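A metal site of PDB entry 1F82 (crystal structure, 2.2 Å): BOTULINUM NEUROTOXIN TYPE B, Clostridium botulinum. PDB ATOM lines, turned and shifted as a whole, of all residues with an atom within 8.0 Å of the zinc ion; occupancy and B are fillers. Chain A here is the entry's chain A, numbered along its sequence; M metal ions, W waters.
Glu 230 touches the zinc ion (OE1 to ZN, 3.9 Å). Within 4 Å of the zinc ion: His 229, Glu 230, His 233 and Glu 267. The nearest printed residue that does not touch the zinc ion is Tyr 372 (4.3 Å).
ND1 of His 233 sits close to OG1 of Thr 270 (3.3 Å). A ring nitrogen (ND1) of His 233 is in hydrogen-bond range of the side-chain carboxylate (OE2) of Glu 266, 3.0 Å away. ND1 of His 229 is in hydrogen-bond range of OE1 of Glu 357, at 2.7 Å. OG1 of Thr 171 is in hydrogen-bond range of OE2 of Glu 230, at 2.8 Å.
Water W1 is bound to the zinc ion, at 2.1 Å. The zinc ion is bound by a ring nitrogen (NE2) of His 233 (2.1 Å). The zinc ion is bound by NE2 of His 229, 2.1 Å away. The zinc ion is bound by OE2 of Glu 267, at 2.2 Å. The zinc ion is bound by OE1 of Glu 267. The zinc ion has five donor atoms within binding distance.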
ATOM      1  N   ASN A 169       0.725   8.629 -11.102  1.00  0.00           N
ATOM      2  CA  ASN A 169       1.133   9.150  -9.797  1.00  0.00           C
ATOM      3  C   ASN A 169       0.530   8.283  -8.701  1.00  0.00           C
ATOM      4  O   ASN A 169      -0.625   7.872  -8.803  1.00  0.00           O
ATOM      5  CB  ASN A 169       0.636  10.579  -9.636  1.00  0.00           C
ATOM      6  CG  ASN A 169       1.019  11.463 -10.791  1.00  0.00           C
ATOM      7  OD1 ASN A 169       2.197  11.758 -10.985  1.00  0.00           O
ATOM      8  ND2 ASN A 169       0.025  11.871 -11.571  1.00  0.00           N
ATOM      9  N   GLU A 170       1.293   8.002  -7.653  1.00  0.00           N
ATOM     10  CA  GLU A 170       0.795   7.166  -6.564  1.00  0.00           C
ATOM     11  C   GLU A 170       1.448   7.478  -5.228  1.00  0.00           C
ATOM     12  O   GLU A 170       2.601   7.923  -5.171  1.00  0.00           O
ATOM     13  CB  GLU A 170       1.006   5.693  -6.905  1.00  0.00           C
ATOM     14  CG  GLU A 170       0.596   4.720  -5.814  1.00  0.00           C
ATOM     15  CD  GLU A 170       0.969   3.279  -6.164  1.00  0.00           C
ATOM     16  OE1 GLU A 170       0.692   2.362  -5.353  1.00  0.00           O
ATOM     17  OE2 GLU A 170       1.536   3.075  -7.254  1.00  0.00           O
ATOM     18  N   THR A 171       0.704   7.271  -4.152  1.00  0.00           N
ATOM     19  CA  THR A 171       1.203   7.482  -2.797  1.00  0.00           C
ATOM     20  C   THR A 171       1.467   6.074  -2.294  1.00  0.00           C
ATOM     21  O   THR A 171       0.645   5.188  -2.493  1.00  0.00           O
ATOM     22  CB  THR A 171       0.169   8.172  -1.931  1.00  0.00           C
ATOM     23  OG1 THR A 171       0.057   9.536  -2.340  1.00  0.00           O
ATOM     24  CG2 THR A 171       0.584   8.130  -0.468  1.00  0.00           C
ATOM     25  N   ILE A 226      -3.778  17.967  -8.419  1.00  0.00           N
ATOM     26  CA  ILE A 226      -3.401  16.572  -8.560  1.00  0.00           C
ATOM     27  C   ILE A 226      -2.499  16.230  -7.395  1.00  0.00           C
ATOM     28  O   ILE A 226      -2.699  15.223  -6.732  1.00  0.00           O
ATOM     29  CB  ILE A 226      -2.662  16.379  -9.884  1.00  0.00           C
ATOM     30  CG1 ILE A 226      -3.652  16.568 -11.026  1.00  0.00           C
ATOM     31  CG2 ILE A 226      -1.994  15.016  -9.933  1.00  0.00           C
ATOM     32  CD1 ILE A 226      -3.083  16.315 -12.371  1.00  0.00           C
ATOM     33  N   HIS A 229      -4.186  16.058  -4.104  1.00  0.00           N
ATOM     34  CA  HIS A 229      -4.974  14.845  -3.990  1.00  0.00           C
ATOM     35  C   HIS A 229      -4.105  13.829  -3.293  1.00  0.00           C
ATOM     36  O   HIS A 229      -4.518  13.229  -2.306  1.00  0.00           O
ATOM     37  CB  HIS A 229      -5.332  14.282  -5.355  1.00  0.00           C
ATOM     38  CG  HIS A 229      -6.078  12.989  -5.302  1.00  0.00           C
ATOM     39  ND1 HIS A 229      -7.420  12.891  -5.597  1.00  0.00           N
ATOM     40  CD2 HIS A 229      -5.680  11.733  -4.990  1.00  0.00           C
ATOM     41  CE1 HIS A 229      -7.811  11.637  -5.476  1.00  0.00           C
ATOM     42  NE2 HIS A 229      -6.771  10.915  -5.112  1.00  0.00           N
ATOM     43  N   GLU A 230      -2.896  13.647  -3.802  1.00  0.00           N
ATOM     44  CA  GLU A 230      -1.960  12.691  -3.220  1.00  0.00           C
ATOM     45  C   GLU A 230      -1.625  13.090  -1.800  1.00  0.00           C
ATOM     46  O   GLU A 230      -1.526  12.256  -0.897  1.00  0.00           O
ATOM     47  CB  GLU A 230      -0.689  12.622  -4.052  1.00  0.00           C
ATOM     48  CG  GLU A 230      -0.944  12.147  -5.469  1.00  0.00           C
ATOM     49  CD  GLU A 230      -1.699  10.835  -5.508  1.00  0.00           C
ATOM     50  OE1 GLU A 230      -2.759  10.769  -6.168  1.00  0.00           O
ATOM     51  OE2 GLU A 230      -1.235   9.873  -4.853  1.00  0.00           O
ATOM     52  N   LEU A 231      -1.454  14.384  -1.586  1.00  0.00           N
ATOM     53  CA  LEU A 231      -1.129  14.829  -0.263  1.00  0.00           C
ATOM     54  C   LEU A 231      -2.232  14.409   0.713  1.00  0.00           C
ATOM     55  O   LEU A 231      -1.983  14.202   1.894  1.00  0.00           O
ATOM     56  CB  LEU A 231      -0.924  16.348  -0.255  1.00  0.00           C
ATOM     57  CG  LEU A 231       0.324  16.817  -1.025  1.00  0.00           C
ATOM     58  CD1 LEU A 231       0.491  18.291  -0.855  1.00  0.00           C
ATOM     59  CD2 LEU A 231       1.565  16.104  -0.504  1.00  0.00           C
ATOM     60  N   ILE A 232      -3.463  14.267   0.241  1.00  0.00           N
ATOM     61  CA  ILE A 232      -4.496  13.857   1.170  1.00  0.00           C
ATOM     62  C   ILE A 232      -4.221  12.402   1.533  1.00  0.00           C
ATOM     63  O   ILE A 232      -4.379  12.001   2.673  1.00  0.00           O
ATOM     64  CB  ILE A 232      -5.920  14.033   0.586  1.00  0.00           C
ATOM     65  CG1 ILE A 232      -6.247  15.531   0.519  1.00  0.00           C
ATOM     66  CG2 ILE A 232      -6.956  13.301   1.446  1.00  0.00           C
ATOM     67  CD1 ILE A 232      -7.609  15.849  -0.023  1.00  0.00           C
ATOM     68  N   HIS A 233      -3.760  11.618   0.574  1.00  0.00           N
ATOM     69  CA  HIS A 233      -3.451  10.227   0.868  1.00  0.00           C
ATOM     70  C   HIS A 233      -2.388  10.208   1.930  1.00  0.00           C
ATOM     71  O   HIS A 233      -2.473   9.483   2.919  1.00  0.00           O
ATOM     72  CB  HIS A 233      -2.955   9.480  -0.362  1.00  0.00           C
ATOM     73  CG  HIS A 233      -4.038   9.138  -1.337  1.00  0.00           C
ATOM     74  ND1 HIS A 233      -5.206   8.505  -0.952  1.00  0.00           N
ATOM     75  CD2 HIS A 233      -4.134   9.334  -2.672  1.00  0.00           C
ATOM     76  CE1 HIS A 233      -5.968   8.325  -2.013  1.00  0.00           C
ATOM     77  NE2 HIS A 233      -5.343   8.816  -3.070  1.00  0.00           N
ATOM     78  N   ILE A 263     -14.293   1.257  -7.085  1.00  0.00           N
ATOM     79  CA  ILE A 263     -13.197   2.144  -6.684  1.00  0.00           C
ATOM     80  C   ILE A 263     -12.835   1.841  -5.219  1.00  0.00           C
ATOM     81  O   ILE A 263     -13.679   1.416  -4.422  1.00  0.00           O
ATOM     82  CB  ILE A 263     -13.631   3.637  -6.795  1.00  0.00           C
ATOM     83  CG1 ILE A 263     -14.191   3.944  -8.181  1.00  0.00           C
ATOM     84  CG2 ILE A 263     -12.454   4.536  -6.529  1.00  0.00           C
ATOM     85  CD1 ILE A 263     -13.194   3.810  -9.314  1.00  0.00           C
ATOM     86  N   GLN A 264     -11.579   2.058  -4.850  1.00  0.00           N
ATOM     87  CA  GLN A 264     -11.134   1.823  -3.478  1.00  0.00           C
ATOM     88  C   GLN A 264     -11.749   2.870  -2.575  1.00  0.00           C
ATOM     89  O   GLN A 264     -11.865   4.042  -2.958  1.00  0.00           O
ATOM     90  CB  GLN A 264      -9.613   1.918  -3.383  1.00  0.00           C
ATOM     91  CG  GLN A 264      -8.871   0.695  -3.858  1.00  0.00           C
ATOM     92  CD  GLN A 264      -8.977  -0.447  -2.875  1.00  0.00           C
ATOM     93  OE1 GLN A 264      -8.488  -1.540  -3.140  1.00  0.00           O
ATOM     94  NE2 GLN A 264      -9.615  -0.204  -1.736  1.00  0.00           N
ATOM     95  N   GLU A 266     -10.554   4.307  -0.013  1.00  0.00           N
ATOM     96  CA  GLU A 266      -9.557   5.347   0.195  1.00  0.00           C
ATOM     97  C   GLU A 266      -9.685   6.424  -0.870  1.00  0.00           C
ATOM     98  O   GLU A 266      -9.510   7.611  -0.578  1.00  0.00           O
ATOM     99  CB  GLU A 266      -8.160   4.729   0.131  1.00  0.00           C
ATOM    100  CG  GLU A 266      -6.995   5.717   0.226  1.00  0.00           C
ATOM    101  CD  GLU A 266      -6.895   6.431   1.569  1.00  0.00           C
ATOM    102  OE1 GLU A 266      -7.036   5.753   2.630  1.00  0.00           O
ATOM    103  OE2 GLU A 266      -6.649   7.661   1.567  1.00  0.00           O
ATOM    104  N   GLU A 267     -10.002   6.031  -2.094  1.00  0.00           N
ATOM    105  CA  GLU A 267     -10.142   7.010  -3.161  1.00  0.00           C
ATOM    106  C   GLU A 267     -11.428   7.825  -3.044  1.00  0.00           C
ATOM    107  O   GLU A 267     -11.457   9.014  -3.348  1.00  0.00           O
ATOM    108  CB  GLU A 267     -10.067   6.319  -4.520  1.00  0.00           C
ATOM    109  CG  GLU A 267      -8.704   5.712  -4.819  1.00  0.00           C
ATOM    110  CD  GLU A 267      -7.609   6.764  -4.965  1.00  0.00           C
ATOM    111  OE1 GLU A 267      -6.447   6.381  -5.216  1.00  0.00           O
ATOM    112  OE2 GLU A 267      -7.919   7.961  -4.840  1.00  0.00           O
ATOM    113  N   LEU A 268     -12.503   7.181  -2.592  1.00  0.00           N
ATOM    114  CA  LEU A 268     -13.779   7.870  -2.472  1.00  0.00           C
ATOM    115  C   LEU A 268     -13.763   8.964  -1.409  1.00  0.00           C
ATOM    116  O   LEU A 268     -14.353  10.026  -1.610  1.00  0.00           O
ATOM    117  CB  LEU A 268     -14.901   6.841  -2.221  1.00  0.00           C
ATOM    118  CG  LEU A 268     -15.155   5.855  -3.381  1.00  0.00           C
ATOM    119  CD1 LEU A 268     -16.217   4.841  -2.999  1.00  0.00           C
ATOM    120  CD2 LEU A 268     -15.593   6.619  -4.630  1.00  0.00           C
ATOM    121  N   THR A 270     -10.909  10.492  -0.269  1.00  0.00           N
ATOM    122  CA  THR A 270      -9.946  11.465  -0.713  1.00  0.00           C
ATOM    123  C   THR A 270     -10.608  12.384  -1.735  1.00  0.00           C
ATOM    124  O   THR A 270     -10.439  13.599  -1.684  1.00  0.00           O
ATOM    125  CB  THR A 270      -8.724  10.791  -1.363  1.00  0.00           C
ATOM    126  OG1 THR A 270      -8.156   9.843  -0.455  1.00  0.00           O
ATOM    127  CG2 THR A 270      -7.655  11.834  -1.699  1.00  0.00           C
ATOM    128  N   PHE A 271     -11.395  11.805  -2.639  1.00  0.00           N
ATOM    129  CA  PHE A 271     -12.041  12.643  -3.651  1.00  0.00           C
ATOM    130  C   PHE A 271     -13.099  13.540  -3.036  1.00  0.00           C
ATOM    131  O   PHE A 271     -13.228  14.712  -3.401  1.00  0.00           O
ATOM    132  CB  PHE A 271     -12.700  11.808  -4.747  1.00  0.00           C
ATOM    133  CG  PHE A 271     -13.285  12.644  -5.841  1.00  0.00           C
ATOM    134  CD1 PHE A 271     -12.467  13.142  -6.856  1.00  0.00           C
ATOM    135  CD2 PHE A 271     -14.621  13.011  -5.806  1.00  0.00           C
ATOM    136  CE1 PHE A 271     -12.985  13.998  -7.824  1.00  0.00           C
ATOM    137  CE2 PHE A 271     -15.146  13.863  -6.768  1.00  0.00           C
ATOM    138  CZ  PHE A 271     -14.328  14.352  -7.772  1.00  0.00           C
ATOM    139  N   GLU A 357     -10.714  16.340  -2.534  1.00  0.00           N
ATOM    140  CA  GLU A 357     -10.379  16.936  -3.837  1.00  0.00           C
ATOM    141  C   GLU A 357     -11.432  17.964  -4.213  1.00  0.00           C
ATOM    142  O   GLU A 357     -11.123  19.096  -4.640  1.00  0.00           O
ATOM    143  CB  GLU A 357     -10.298  15.870  -4.936  1.00  0.00           C
ATOM    144  CG  GLU A 357      -9.657  16.417  -6.224  1.00  0.00           C
ATOM    145  CD  GLU A 357      -9.600  15.413  -7.373  1.00  0.00           C
ATOM    146  OE1 GLU A 357      -9.184  14.253  -7.142  1.00  0.00           O
ATOM    147  OE2 GLU A 357      -9.943  15.793  -8.521  1.00  0.00           O
ATOM    148  N   ARG A 369     -13.170  16.929 -12.151  1.00  0.00           N
ATOM    149  CA  ARG A 369     -14.286  16.037 -12.510  1.00  0.00           C
ATOM    150  C   ARG A 369     -15.403  16.052 -11.486  1.00  0.00           C
ATOM    151  O   ARG A 369     -15.248  16.592 -10.395  1.00  0.00           O
ATOM    152  CB  ARG A 369     -13.795  14.587 -12.695  1.00  0.00           C
ATOM    153  CG  ARG A 369     -12.982  14.019 -11.544  1.00  0.00           C
ATOM    154  CD  ARG A 369     -11.528  14.452 -11.655  1.00  0.00           C
ATOM    155  NE  ARG A 369     -10.681  13.923 -10.591  1.00  0.00           N
ATOM    156  CZ  ARG A 369     -10.426  12.626 -10.392  1.00  0.00           C
ATOM    157  NH1 ARG A 369     -10.978  11.706 -11.187  1.00  0.00           N
ATOM    158  NH2 ARG A 369      -9.627  12.261  -9.399  1.00  0.00           N
ATOM    159  N   TYR A 372     -15.006  10.513  -8.761  1.00  0.00           N
ATOM    160  CA  TYR A 372     -13.807   9.714  -8.968  1.00  0.00           C
ATOM    161  C   TYR A 372     -14.191   8.662  -9.987  1.00  0.00           C
ATOM    162  O   TYR A 372     -13.343   8.001 -10.571  1.00  0.00           O
ATOM    163  CB  TYR A 372     -13.349   9.043  -7.678  1.00  0.00           C
ATOM    164  CG  TYR A 372     -11.934   8.537  -7.809  1.00  0.00           C
ATOM    165  CD1 TYR A 372     -11.667   7.186  -8.045  1.00  0.00           C
ATOM    166  CD2 TYR A 372     -10.861   9.422  -7.796  1.00  0.00           C
ATOM    167  CE1 TYR A 372     -10.347   6.732  -8.267  1.00  0.00           C
ATOM    168  CE2 TYR A 372      -9.556   8.992  -7.999  1.00  0.00           C
ATOM    169  CZ  TYR A 372      -9.303   7.649  -8.246  1.00  0.00           C
ATOM    170  OH  TYR A 372      -7.998   7.252  -8.460  1.00  0.00           O
HETATM  171 ZN    ZN M   1      -5.961   8.924  -5.082  1.00  0.00          ZN
HETATM  172  O   HOH W   1      -4.211   8.372  -6.065  1.00  0.00           O
